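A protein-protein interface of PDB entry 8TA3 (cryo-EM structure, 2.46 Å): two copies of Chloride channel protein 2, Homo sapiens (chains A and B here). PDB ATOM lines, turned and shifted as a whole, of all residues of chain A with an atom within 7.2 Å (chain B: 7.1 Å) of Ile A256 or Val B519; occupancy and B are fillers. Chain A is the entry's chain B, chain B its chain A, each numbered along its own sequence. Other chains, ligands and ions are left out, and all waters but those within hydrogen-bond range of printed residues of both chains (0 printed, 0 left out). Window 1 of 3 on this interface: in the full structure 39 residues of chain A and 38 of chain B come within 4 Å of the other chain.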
ATOM      1  N   GLY A 249     -37.790  -8.185   9.563  1.00  0.00           N
ATOM      2  CA  GLY A 249     -38.019  -9.508   8.983  1.00  0.00           C
ATOM      3  C   GLY A 249     -39.450  -9.725   8.485  1.00  0.00           C
ATOM      4  O   GLY A 249     -39.632 -10.238   7.384  1.00  0.00           O
ATOM      5  N   ALA A 253     -40.375 -10.158   4.411  1.00  0.00           N
ATOM      6  CA  ALA A 253     -40.389 -11.627   4.417  1.00  0.00           C
ATOM      7  C   ALA A 253     -38.985 -12.241   4.202  1.00  0.00           C
ATOM      8  O   ALA A 253     -38.819 -13.246   3.513  1.00  0.00           O
ATOM      9  CB  ALA A 253     -41.478 -12.166   3.481  1.00  0.00           C
ATOM     10  N   ALA A 254     -37.969 -11.609   4.793  1.00  0.00           N
ATOM     11  CA  ALA A 254     -36.547 -11.891   4.633  1.00  0.00           C
ATOM     12  C   ALA A 254     -35.894 -12.105   6.013  1.00  0.00           C
ATOM     13  O   ALA A 254     -35.355 -11.156   6.590  1.00  0.00           O
ATOM     14  CB  ALA A 254     -35.932 -10.723   3.847  1.00  0.00           C
ATOM     15  N   PRO A 255     -36.010 -13.304   6.612  1.00  0.00           N
ATOM     16  CA  PRO A 255     -35.585 -13.565   7.983  1.00  0.00           C
ATOM     17  C   PRO A 255     -34.122 -13.249   8.314  1.00  0.00           C
ATOM     18  O   PRO A 255     -33.874 -12.669   9.359  1.00  0.00           O
ATOM     19  CB  PRO A 255     -35.876 -15.041   8.227  1.00  0.00           C
ATOM     20  CG  PRO A 255     -37.039 -15.319   7.296  1.00  0.00           C
ATOM     21  CD  PRO A 255     -36.703 -14.467   6.084  1.00  0.00           C
ATOM     22  N   ILE A 256     -33.139 -13.592   7.478  1.00  0.00           N
ATOM     23  CA  ILE A 256     -31.722 -13.370   7.812  1.00  0.00           C
ATOM     24  C   ILE A 256     -31.316 -11.920   7.532  1.00  0.00           C
ATOM     25  O   ILE A 256     -30.717 -11.266   8.382  1.00  0.00           O
ATOM     26  CB  ILE A 256     -30.816 -14.399   7.088  1.00  0.00           C
ATOM     27  CG1 ILE A 256     -31.180 -15.826   7.554  1.00  0.00           C
ATOM     28  CG2 ILE A 256     -29.328 -14.117   7.356  1.00  0.00           C
ATOM     29  CD1 ILE A 256     -30.376 -16.959   6.910  1.00  0.00           C
ATOM     30  N   GLY A 257     -31.683 -11.375   6.375  1.00  0.00           N
ATOM     31  CA  GLY A 257     -31.388 -10.010   5.976  1.00  0.00           C
ATOM     32  C   GLY A 257     -32.064  -8.980   6.873  1.00  0.00           C
ATOM     33  O   GLY A 257     -31.443  -7.977   7.204  1.00  0.00           O
ATOM     34  N   GLY A 258     -33.285  -9.251   7.342  1.00  0.00           N
ATOM     35  CA  GLY A 258     -33.996  -8.411   8.296  1.00  0.00           C
ATOM     36  C   GLY A 258     -33.323  -8.309   9.665  1.00  0.00           C
ATOM     37  O   GLY A 258     -33.171  -7.212  10.196  1.00  0.00           O
ATOM     38  N   VAL A 259     -32.833  -9.426  10.211  1.00  0.00           N
ATOM     39  CA  VAL A 259     -32.023  -9.435  11.443  1.00  0.00           C
ATOM     40  C   VAL A 259     -30.732  -8.633  11.255  1.00  0.00           C
ATOM     41  O   VAL A 259     -30.461  -7.731  12.044  1.00  0.00           O
ATOM     42  CB  VAL A 259     -31.719 -10.868  11.917  1.00  0.00           C
ATOM     43  CG1 VAL A 259     -30.837 -10.904  13.168  1.00  0.00           C
ATOM     44  CG2 VAL A 259     -32.990 -11.649  12.262  1.00  0.00           C
ATOM     45  N   LEU A 260     -29.964  -8.879  10.192  1.00  0.00           N
ATOM     46  CA  LEU A 260     -28.709  -8.167   9.929  1.00  0.00           C
ATOM     47  C   LEU A 260     -28.894  -6.667   9.657  1.00  0.00           C
ATOM     48  O   LEU A 260     -28.117  -5.863  10.161  1.00  0.00           O
ATOM     49  CB  LEU A 260     -27.968  -8.828   8.758  1.00  0.00           C
ATOM     50  CG  LEU A 260     -27.527 -10.282   8.980  1.00  0.00           C
ATOM     51  CD1 LEU A 260     -27.015 -10.852   7.659  1.00  0.00           C
ATOM     52  CD2 LEU A 260     -26.431 -10.392  10.033  1.00  0.00           C
ATOM     53  N   PHE A 261     -29.933  -6.261   8.918  1.00  0.00           N
ATOM     54  CA  PHE A 261     -30.266  -4.852   8.680  1.00  0.00           C
ATOM     55  C   PHE A 261     -30.671  -4.135   9.974  1.00  0.00           C
ATOM     56  O   PHE A 261     -30.184  -3.042  10.247  1.00  0.00           O
ATOM     57  CB  PHE A 261     -31.362  -4.771   7.603  1.00  0.00           C
ATOM     58  CG  PHE A 261     -31.852  -3.374   7.256  1.00  0.00           C
ATOM     59  CD1 PHE A 261     -32.856  -2.761   8.028  1.00  0.00           C
ATOM     60  CD2 PHE A 261     -31.306  -2.674   6.167  1.00  0.00           C
ATOM     61  CE1 PHE A 261     -33.311  -1.470   7.718  1.00  0.00           C
ATOM     62  CE2 PHE A 261     -31.752  -1.377   5.860  1.00  0.00           C
ATOM     63  CZ  PHE A 261     -32.755  -0.776   6.635  1.00  0.00           C
ATOM     64  N   SER A 262     -31.500  -4.758  10.819  1.00  0.00           N
ATOM     65  CA  SER A 262     -31.881  -4.178  12.116  1.00  0.00           C
ATOM     66  C   SER A 262     -30.684  -3.939  13.046  1.00  0.00           C
ATOM     67  O   SER A 262     -30.650  -2.931  13.746  1.00  0.00           O
ATOM     68  CB  SER A 262     -32.919  -5.054  12.808  1.00  0.00           C
ATOM     69  OG  SER A 262     -32.319  -6.185  13.392  1.00  0.00           O
ATOM     70  N   TYR A 275     -27.957 -11.432  18.286  1.00  0.00           N
ATOM     71  CA  TYR A 275     -28.067 -12.015  16.944  1.00  0.00           C
ATOM     72  C   TYR A 275     -28.740 -13.397  16.976  1.00  0.00           C
ATOM     73  O   TYR A 275     -29.644 -13.641  16.179  1.00  0.00           O
ATOM     74  CB  TYR A 275     -26.687 -12.037  16.273  1.00  0.00           C
ATOM     75  CG  TYR A 275     -26.552 -12.845  14.989  1.00  0.00           C
ATOM     76  CD1 TYR A 275     -27.379 -12.586  13.879  1.00  0.00           C
ATOM     77  CD2 TYR A 275     -25.545 -13.820  14.878  1.00  0.00           C
ATOM     78  CE1 TYR A 275     -27.217 -13.307  12.677  1.00  0.00           C
ATOM     79  CE2 TYR A 275     -25.362 -14.520  13.671  1.00  0.00           C
ATOM     80  CZ  TYR A 275     -26.194 -14.271  12.564  1.00  0.00           C
ATOM     81  OH  TYR A 275     -25.987 -14.942  11.395  1.00  0.00           O
ATOM     82  N   PHE A 279     -32.427 -14.111  15.330  1.00  0.00           N
ATOM     83  CA  PHE A 279     -32.526 -15.227  14.376  1.00  0.00           C
ATOM     84  C   PHE A 279     -33.585 -16.258  14.803  1.00  0.00           C
ATOM     85  O   PHE A 279     -34.374 -16.729  13.981  1.00  0.00           O
ATOM     86  CB  PHE A 279     -31.123 -15.843  14.225  1.00  0.00           C
ATOM     87  CG  PHE A 279     -30.863 -16.769  13.044  1.00  0.00           C
ATOM     88  CD1 PHE A 279     -31.492 -18.024  12.940  1.00  0.00           C
ATOM     89  CD2 PHE A 279     -29.921 -16.402  12.065  1.00  0.00           C
ATOM     90  CE1 PHE A 279     -31.181 -18.898  11.886  1.00  0.00           C
ATOM     91  CE2 PHE A 279     -29.599 -17.278  11.016  1.00  0.00           C
ATOM     92  CZ  PHE A 279     -30.227 -18.528  10.924  1.00  0.00           C
ATOM     93  N   ALA A 282     -37.258 -14.363  14.322  1.00  0.00           N
ATOM     94  CA  ALA A 282     -37.516 -14.239  12.883  1.00  0.00           C
ATOM     95  C   ALA A 282     -37.840 -15.579  12.187  1.00  0.00           C
ATOM     96  O   ALA A 282     -38.668 -15.612  11.283  1.00  0.00           O
ATOM     97  CB  ALA A 282     -36.308 -13.562  12.235  1.00  0.00           C
ATOM     98  N   THR A 283     -37.249 -16.694  12.620  1.00  0.00           N
ATOM     99  CA  THR A 283     -37.552 -18.036  12.092  1.00  0.00           C
ATOM    100  C   THR A 283     -38.987 -18.459  12.412  1.00  0.00           C
ATOM    101  O   THR A 283     -39.678 -19.011  11.558  1.00  0.00           O
ATOM    102  CB  THR A 283     -36.579 -19.093  12.649  1.00  0.00           C
ATOM    103  OG1 THR A 283     -35.251 -18.735  12.386  1.00  0.00           O
ATOM    104  CG2 THR A 283     -36.775 -20.471  12.026  1.00  0.00           C
ATOM    105  N   SER A 516     -26.251  -5.035   4.352  1.00  0.00           N
ATOM    106  CA  SER A 516     -27.196  -6.157   4.419  1.00  0.00           C
ATOM    107  C   SER A 516     -28.375  -6.090   3.439  1.00  0.00           C
ATOM    108  O   SER A 516     -29.133  -7.049   3.349  1.00  0.00           O
ATOM    109  CB  SER A 516     -27.711  -6.342   5.842  1.00  0.00           C
ATOM    110  OG  SER A 516     -26.619  -6.492   6.712  1.00  0.00           O
ATOM    111  N   VAL A 519     -28.139  -9.244   1.300  1.00  0.00           N
ATOM    112  CA  VAL A 519     -28.807 -10.444   1.831  1.00  0.00           C
ATOM    113  C   VAL A 519     -30.330 -10.351   1.669  1.00  0.00           C
ATOM    114  O   VAL A 519     -30.954 -11.310   1.227  1.00  0.00           O
ATOM    115  CB  VAL A 519     -28.392 -10.709   3.294  1.00  0.00           C
ATOM    116  CG1 VAL A 519     -28.992 -12.003   3.845  1.00  0.00           C
ATOM    117  CG2 VAL A 519     -26.871 -10.815   3.433  1.00  0.00           C
ATOM    118  N   ILE A 520     -30.920  -9.174   1.931  1.00  0.00           N
ATOM    119  CA  ILE A 520     -32.353  -8.900   1.709  1.00  0.00           C
ATOM    120  C   ILE A 520     -32.753  -9.171   0.251  1.00  0.00           C
ATOM    121  O   ILE A 520     -33.770  -9.811   0.012  1.00  0.00           O
ATOM    122  CB  ILE A 520     -32.741  -7.461   2.154  1.00  0.00           C
ATOM    123  CG1 ILE A 520     -32.643  -7.332   3.686  1.00  0.00           C
ATOM    124  CG2 ILE A 520     -34.160  -7.060   1.700  1.00  0.00           C
ATOM    125  CD1 ILE A 520     -32.632  -5.889   4.196  1.00  0.00           C
ATOM    126  N   GLU A 523     -33.159 -12.921  -0.496  1.00  0.00           N
ATOM    127  CA  GLU A 523     -34.372 -13.443   0.133  1.00  0.00           C
ATOM    128  C   GLU A 523     -35.661 -12.931  -0.520  1.00  0.00           C
ATOM    129  O   GLU A 523     -36.597 -13.710  -0.666  1.00  0.00           O
ATOM    130  CB  GLU A 523     -34.354 -13.126   1.629  1.00  0.00           C
ATOM    131  CG  GLU A 523     -33.354 -14.003   2.384  1.00  0.00           C
ATOM    132  CD  GLU A 523     -33.268 -13.610   3.868  1.00  0.00           C
ATOM    133  OE1 GLU A 523     -32.829 -12.485   4.165  1.00  0.00           O
ATOM    134  OE2 GLU A 523     -33.646 -14.414   4.745  1.00  0.00           O
ATOM    135  N   ILE A 528     -29.729 -16.547  -5.709  1.00  0.00           N
ATOM    136  CA  ILE A 528     -28.410 -16.055  -5.261  1.00  0.00           C
ATOM    137  C   ILE A 528     -27.352 -16.077  -6.385  1.00  0.00           C
ATOM    138  O   ILE A 528     -26.160 -15.961  -6.142  1.00  0.00           O
ATOM    139  CB  ILE A 528     -28.031 -16.738  -3.917  1.00  0.00           C
ATOM    140  CG1 ILE A 528     -26.911 -16.002  -3.151  1.00  0.00           C
ATOM    141  CG2 ILE A 528     -27.685 -18.221  -4.081  1.00  0.00           C
ATOM    142  CD1 ILE A 528     -26.835 -16.383  -1.671  1.00  0.00           C
ATOM    143  N   ILE A 531     -24.753 -12.841  -6.847  1.00  0.00           N
ATOM    144  CA  ILE A 531     -24.066 -12.464  -5.605  1.00  0.00           C
ATOM    145  C   ILE A 531     -22.805 -11.609  -5.790  1.00  0.00           C
ATOM    146  O   ILE A 531     -22.654 -10.619  -5.082  1.00  0.00           O
ATOM    147  CB  ILE A 531     -23.826 -13.704  -4.718  1.00  0.00           C
ATOM    148  CG1 ILE A 531     -23.196 -13.273  -3.382  1.00  0.00           C
ATOM    149  CG2 ILE A 531     -22.964 -14.792  -5.375  1.00  0.00           C
ATOM    150  CD1 ILE A 531     -23.366 -14.293  -2.270  1.00  0.00           C
ATOM    151  N   ALA B 254     -17.195 -18.333   0.111  1.00  0.00           N
ATOM    152  CA  ALA B 254     -18.497 -17.916   0.638  1.00  0.00           C
ATOM    153  C   ALA B 254     -18.379 -16.512   1.268  1.00  0.00           C
ATOM    154  O   ALA B 254     -18.127 -16.391   2.471  1.00  0.00           O
ATOM    155  CB  ALA B 254     -18.987 -18.992   1.613  1.00  0.00           C
ATOM    156  N   PRO B 255     -18.439 -15.437   0.462  1.00  0.00           N
ATOM    157  CA  PRO B 255     -18.047 -14.094   0.879  1.00  0.00           C
ATOM    158  C   PRO B 255     -18.852 -13.459   2.025  1.00  0.00           C
ATOM    159  O   PRO B 255     -18.257 -12.735   2.809  1.00  0.00           O
ATOM    160  CB  PRO B 255     -18.154 -13.232  -0.380  1.00  0.00           C
ATOM    161  CG  PRO B 255     -17.942 -14.225  -1.505  1.00  0.00           C
ATOM    162  CD  PRO B 255     -18.655 -15.455  -0.979  1.00  0.00           C
ATOM    163  N   ILE B 256     -20.163 -13.686   2.154  1.00  0.00           N
ATOM    164  CA  ILE B 256     -20.969 -13.115   3.251  1.00  0.00           C
ATOM    165  C   ILE B 256     -20.959 -14.042   4.467  1.00  0.00           C
ATOM    166  O   ILE B 256     -20.710 -13.602   5.589  1.00  0.00           O
ATOM    167  CB  ILE B 256     -22.415 -12.783   2.797  1.00  0.00           C
ATOM    168  CG1 ILE B 256     -22.386 -11.776   1.629  1.00  0.00           C
ATOM    169  CG2 ILE B 256     -23.254 -12.229   3.969  1.00  0.00           C
ATOM    170  CD1 ILE B 256     -23.760 -11.397   1.068  1.00  0.00           C
ATOM    171  N   GLY B 257     -21.184 -15.338   4.267  1.00  0.00           N
ATOM    172  CA  GLY B 257     -21.267 -16.330   5.331  1.00  0.00           C
ATOM    173  C   GLY B 257     -19.966 -16.487   6.108  1.00  0.00           C
ATOM    174  O   GLY B 257     -20.005 -16.622   7.328  1.00  0.00           O
ATOM    175  N   GLY B 258     -18.810 -16.375   5.449  1.00  0.00           N
ATOM    176  CA  GLY B 258     -17.504 -16.405   6.103  1.00  0.00           C
ATOM    177  C   GLY B 258     -17.233 -15.203   7.010  1.00  0.00           C
ATOM    178  O   GLY B 258     -16.669 -15.361   8.090  1.00  0.00           O
ATOM    179  N   LEU B 260     -19.768 -13.415   8.589  1.00  0.00           N
ATOM    180  CA  LEU B 260     -20.675 -13.642   9.718  1.00  0.00           C
ATOM    181  C   LEU B 260     -20.195 -14.756  10.668  1.00  0.00           C
ATOM    182  O   LEU B 260     -20.220 -14.565  11.877  1.00  0.00           O
ATOM    183  CB  LEU B 260     -22.093 -13.945   9.199  1.00  0.00           C
ATOM    184  CG  LEU B 260     -22.767 -12.828   8.380  1.00  0.00           C
ATOM    185  CD1 LEU B 260     -24.089 -13.338   7.824  1.00  0.00           C
ATOM    186  CD2 LEU B 260     -23.039 -11.586   9.214  1.00  0.00           C
ATOM    187  N   ALA B 505     -25.557 -28.241   7.281  1.00  0.00           N
ATOM    188  CA  ALA B 505     -25.585 -26.968   7.988  1.00  0.00           C
ATOM    189  C   ALA B 505     -25.864 -27.124   9.499  1.00  0.00           C
ATOM    190  O   ALA B 505     -25.246 -26.438  10.310  1.00  0.00           O
ATOM    191  CB  ALA B 505     -26.630 -26.079   7.308  1.00  0.00           C
ATOM    192  N   VAL B 515     -24.959 -19.881  13.996  1.00  0.00           N
ATOM    193  CA  VAL B 515     -26.147 -19.901  13.116  1.00  0.00           C
ATOM    194  C   VAL B 515     -25.803 -19.550  11.669  1.00  0.00           C
ATOM    195  O   VAL B 515     -26.533 -19.911  10.757  1.00  0.00           O
ATOM    196  CB  VAL B 515     -27.312 -19.046  13.652  1.00  0.00           C
ATOM    197  CG1 VAL B 515     -27.818 -19.560  15.001  1.00  0.00           C
ATOM    198  CG2 VAL B 515     -26.967 -17.567  13.761  1.00  0.00           C
ATOM    199  N   SER B 516     -24.649 -18.927  11.430  1.00  0.00           N
ATOM    200  CA  SER B 516     -24.197 -18.509  10.097  1.00  0.00           C
ATOM    201  C   SER B 516     -23.820 -19.645   9.141  1.00  0.00           C
ATOM    202  O   SER B 516     -23.620 -19.390   7.957  1.00  0.00           O
ATOM    203  CB  SER B 516     -23.034 -17.535  10.217  1.00  0.00           C
ATOM    204  OG  SER B 516     -23.416 -16.484  11.067  1.00  0.00           O
ATOM    205  N   THR B 517     -23.796 -20.905   9.588  1.00  0.00           N
ATOM    206  CA  THR B 517     -23.709 -22.060   8.676  1.00  0.00           C
ATOM    207  C   THR B 517     -24.884 -22.147   7.697  1.00  0.00           C
ATOM    208  O   THR B 517     -24.716 -22.706   6.620  1.00  0.00           O
ATOM    209  CB  THR B 517     -23.581 -23.400   9.410  1.00  0.00           C
ATOM    210  OG1 THR B 517     -24.699 -23.631  10.223  1.00  0.00           O
ATOM    211  CG2 THR B 517     -22.333 -23.463  10.272  1.00  0.00           C
ATOM    212  N   ALA B 518     -26.039 -21.540   8.003  1.00  0.00           N
ATOM    213  CA  ALA B 518     -27.117 -21.325   7.041  1.00  0.00           C
ATOM    214  C   ALA B 518     -26.672 -20.483   5.829  1.00  0.00           C
ATOM    215  O   ALA B 518     -26.791 -20.924   4.695  1.00  0.00           O
ATOM    216  CB  ALA B 518     -28.301 -20.686   7.775  1.00  0.00           C
ATOM    217  N   VAL B 519     -26.077 -19.307   6.045  1.00  0.00           N
ATOM    218  CA  VAL B 519     -25.586 -18.442   4.955  1.00  0.00           C
ATOM    219  C   VAL B 519     -24.453 -19.103   4.158  1.00  0.00           C
ATOM    220  O   VAL B 519     -24.476 -19.069   2.932  1.00  0.00           O
ATOM    221  CB  VAL B 519     -25.174 -17.060   5.500  1.00  0.00           C
ATOM    222  CG1 VAL B 519     -24.754 -16.091   4.393  1.00  0.00           C
ATOM    223  CG2 VAL B 519     -26.338 -16.407   6.249  1.00  0.00           C
ATOM    224  N   ILE B 520     -23.518 -19.786   4.840  1.00  0.00           N
ATOM    225  CA  ILE B 520     -22.468 -20.594   4.201  1.00  0.00           C
ATOM    226  C   ILE B 520     -23.069 -21.648   3.255  1.00  0.00           C
ATOM    227  O   ILE B 520     -22.620 -21.764   2.120  1.00  0.00           O
ATOM    228  CB  ILE B 520     -21.523 -21.225   5.261  1.00  0.00           C
ATOM    229  CG1 ILE B 520     -20.708 -20.128   5.979  1.00  0.00           C
ATOM    230  CG2 ILE B 520     -20.562 -22.259   4.652  1.00  0.00           C
ATOM    231  CD1 ILE B 520     -19.923 -20.592   7.207  1.00  0.00           C
ATOM    232  N   VAL B 521     -24.102 -22.390   3.662  1.00  0.00           N
ATOM    233  CA  VAL B 521     -24.701 -23.433   2.815  1.00  0.00           C
ATOM    234  C   VAL B 521     -25.371 -22.888   1.544  1.00  0.00           C
ATOM    235  O   VAL B 521     -25.302 -23.535   0.499  1.00  0.00           O
ATOM    236  CB  VAL B 521     -25.608 -24.365   3.651  1.00  0.00           C
ATOM    237  CG1 VAL B 521     -27.121 -24.162   3.537  1.00  0.00           C
ATOM    238  CG2 VAL B 521     -25.295 -25.812   3.287  1.00  0.00           C
ATOM    239  N   PHE B 522     -25.947 -21.683   1.562  1.00  0.00           N
ATOM    240  CA  PHE B 522     -26.482 -21.043   0.352  1.00  0.00           C
ATOM    241  C   PHE B 522     -25.377 -20.610  -0.622  1.00  0.00           C
ATOM    242  O   PHE B 522     -25.495 -20.807  -1.827  1.00  0.00           O
ATOM    243  CB  PHE B 522     -27.371 -19.846   0.721  1.00  0.00           C
ATOM    244  CG  PHE B 522     -28.450 -20.121   1.749  1.00  0.00           C
ATOM    245  CD1 PHE B 522     -29.170 -21.330   1.739  1.00  0.00           C
ATOM    246  CD2 PHE B 522     -28.715 -19.163   2.742  1.00  0.00           C
ATOM    247  CE1 PHE B 522     -30.096 -21.608   2.755  1.00  0.00           C
ATOM    248  CE2 PHE B 522     -29.643 -19.439   3.755  1.00  0.00           C
ATOM    249  CZ  PHE B 522     -30.312 -20.672   3.777  1.00  0.00           C
ATOM    250  N   GLU B 523     -24.269 -20.067  -0.130  1.00  0.00           N
ATOM    251  CA  GLU B 523     -23.143 -19.676  -0.980  1.00  0.00           C
ATOM    252  C   GLU B 523     -22.325 -20.856  -1.528  1.00  0.00           C
ATOM    253  O   GLU B 523     -21.851 -20.775  -2.656  1.00  0.00           O
ATOM    254  CB  GLU B 523     -22.237 -18.709  -0.225  1.00  0.00           C
ATOM    255  CG  GLU B 523     -22.936 -17.378   0.056  1.00  0.00           C
ATOM    256  CD  GLU B 523     -22.051 -16.472   0.915  1.00  0.00           C
ATOM    257  OE1 GLU B 523     -21.724 -16.858   2.055  1.00  0.00           O
ATOM    258  OE2 GLU B 523     -21.666 -15.377   0.453  1.00  0.00           O
ATOM    259  N   LEU B 524     -22.187 -21.972  -0.804  1.00  0.00           N
ATOM    260  CA  LEU B 524     -21.541 -23.194  -1.317  1.00  0.00           C
ATOM    261  C   LEU B 524     -22.349 -23.894  -2.415  1.00  0.00           C
ATOM    262  O   LEU B 524     -21.765 -24.512  -3.300  1.00  0.00           O
ATOM    263  CB  LEU B 524     -21.315 -24.189  -0.165  1.00  0.00           C
ATOM    264  CG  LEU B 524     -20.139 -23.871   0.768  1.00  0.00           C
ATOM    265  CD1 LEU B 524     -20.174 -24.812   1.969  1.00  0.00           C
ATOM    266  CD2 LEU B 524     -18.797 -24.075   0.078  1.00  0.00           C
ATOM    267  N   ILE B 528     -30.948 -20.848  -2.698  1.00  0.00           N
ATOM    268  CA  ILE B 528     -31.533 -20.382  -1.430  1.00  0.00           C
ATOM    269  C   ILE B 528     -32.983 -20.877  -1.252  1.00  0.00           C
ATOM    270  O   ILE B 528     -33.732 -20.391  -0.410  1.00  0.00           O
ATOM    271  CB  ILE B 528     -31.296 -18.856  -1.274  1.00  0.00           C
ATOM    272  CG1 ILE B 528     -31.496 -18.365   0.174  1.00  0.00           C
ATOM    273  CG2 ILE B 528     -32.144 -18.023  -2.247  1.00  0.00           C
ATOM    274  CD1 ILE B 528     -30.796 -17.038   0.464  1.00  0.00           C
ATOM    275  N   ILE B 531     -34.270 -22.297   2.489  1.00  0.00           N
ATOM    276  CA  ILE B 531     -33.967 -21.397   3.615  1.00  0.00           C
ATOM    277  C   ILE B 531     -34.786 -21.639   4.897  1.00  0.00           C
ATOM    278  O   ILE B 531     -34.208 -21.665   5.979  1.00  0.00           O
ATOM    279  CB  ILE B 531     -33.998 -19.922   3.155  1.00  0.00           C
ATOM    280  CG1 ILE B 531     -33.614 -18.990   4.317  1.00  0.00           C
ATOM    281  CG2 ILE B 531     -35.345 -19.488   2.554  1.00  0.00           C
ATOM    282  CD1 ILE B 531     -33.209 -17.593   3.871  1.00  0.00           C
ATOM    283  N   VAL B 534     -33.569 -25.084   6.527  1.00  0.00           N
ATOM    284  CA  VAL B 534     -32.217 -24.858   7.058  1.00  0.00           C
ATOM    285  C   VAL B 534     -32.272 -24.092   8.376  1.00  0.00           C
ATOM    286  O   VAL B 534     -31.707 -24.556   9.360  1.00  0.00           O
ATOM    287  CB  VAL B 534     -31.318 -24.151   6.022  1.00  0.00           C
ATOM    288  CG1 VAL B 534     -29.975 -23.696   6.583  1.00  0.00           C
ATOM    289  CG2 VAL B 534     -30.996 -25.064   4.840  1.00  0.00           C
ATOM    290  N   MET B 535     -32.989 -22.967   8.449  1.00  0.00           N
ATOM    291  CA  MET B 535     -33.107 -22.177   9.680  1.00  0.00           C
ATOM    292  C   MET B 535     -33.812 -22.907  10.828  1.00  0.00           C
ATOM    293  O   MET B 535     -33.375 -22.785  11.965  1.00  0.00           O
ATOM    294  CB  MET B 535     -33.845 -20.871   9.408  1.00  0.00           C
ATOM    295  CG  MET B 535     -33.056 -19.901   8.534  1.00  0.00           C
ATOM    296  SD  MET B 535     -33.971 -18.371   8.253  1.00  0.00           S
ATOM    297  CE  MET B 535     -33.528 -17.463   9.760  1.00  0.00           C
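Printed residues of chain A that touch a printed residue of chain B: Pro A255, Ile A256, Leu A260, Tyr A275, Phe A279, Thr A283, Val A519, Glu A523 and Ile A531.
Hydrophobic or aromatic side chains of chain A that line the printed part of chain B: Pro A255, Ile A256, Leu A260, Tyr A275, Phe A279, Val A519 and Ile A531.
Hydrophobic or aromatic side chains of chain B that line the printed part of chain A: Ile B256, Leu B260, Val B515, Val B519, Ile B531 and Met B535.
Among the printed residues, no Asp or Glu carboxylate lies within 4 Å of a Lys or Arg side-chain nitrogen of the other chain.
The side-chain hydroxyl (OG) of Ser B516 is in hydrogen-bond range of the side-chain hydroxyl (OH) of Tyr A275, 3.0 Å away.
Printed residues of chain B within 4 Å of Pro A255: Met B535.
Ile A256 touches two residues of chain B.
Ile A528 touches none of the printed residues of chain B.
Printed residues of chain B within 4 Å of Ile A531: Glu B523 (3.4 Å).
Of the printed residues of chain A, Val B515 touches Tyr A275 and Phe A279.
Thr B517 touches none of the printed residues of chain A.
Ala B518 touches none of the printed residues of chain A.
Of chain A, only Ile A256 comes within 4 Å of Val B519.
Of the printed residues of chain A, Ile B531 touches Glu A523 (3.3 Å).
The nearest residue of chain B that does not touch Ile A256 is Phe B522 (4.1 Å).
The nearest residue of chain A that does not touch Val B519 is Tyr A275 (5.4 Å).
The nearest printed residue of chain A that does not touch Met B535 is Ala A282 (5.3 Å).
Ile A256 touches Val B519.
CE of Met B535 touches CG1 of Ile A256 (3.6 Å).
Leu B260 touches Leu A260.
CE2 of Tyr A275 touches CG2 of Val B515, 3.4 Å away.
Phe A279 touches Val B515.
CE1 of Phe A279 touches CE of Met B535, 3.5 Å away.
Met B535 touches Thr A283.
Ile B256 touches Val A519 (CG2 to CG2, 3.9 Å).
OE2 of Glu A523 touches CD1 of Ile B531 (3.3 Å).
Ile A531 touches Glu B523 (CD1 to OE2, 3.4 Å).
The backbone NH of Ile B256 sits at hydrogen-bond distance from the side-chain carboxylate of Glu B523.
The backbone NH (N) of Gly B257 is in hydrogen-bond range of the side-chain carboxylate (OE1) of Glu B523, at 2.7 Å.
The backbone NH of Ile A256 sits at hydrogen-bond distance from the side-chain carboxylate of Glu A523 (2.9 Å).
N of Gly A257 lies within hydrogen-bond range of OE1 of Glu A523 (2.7 Å).
The backbone carbonyl oxygen of Phe A279 is in hydrogen-bond range of the side-chain hydroxyl of Thr A283 (2.7 Å).
Ile A256 touches Val B519, and with the chains exchanged Val A519 touches Ile B256.
Leu A260 touches its own counterpart, Leu B260.
Glu A523 touches Ile B531, and with the chains exchanged Ile A531 touches Glu B523.
Of the 12 pairs that touch across the chains among the printed residues, 5 have their exchanged pair printed and touching as well.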
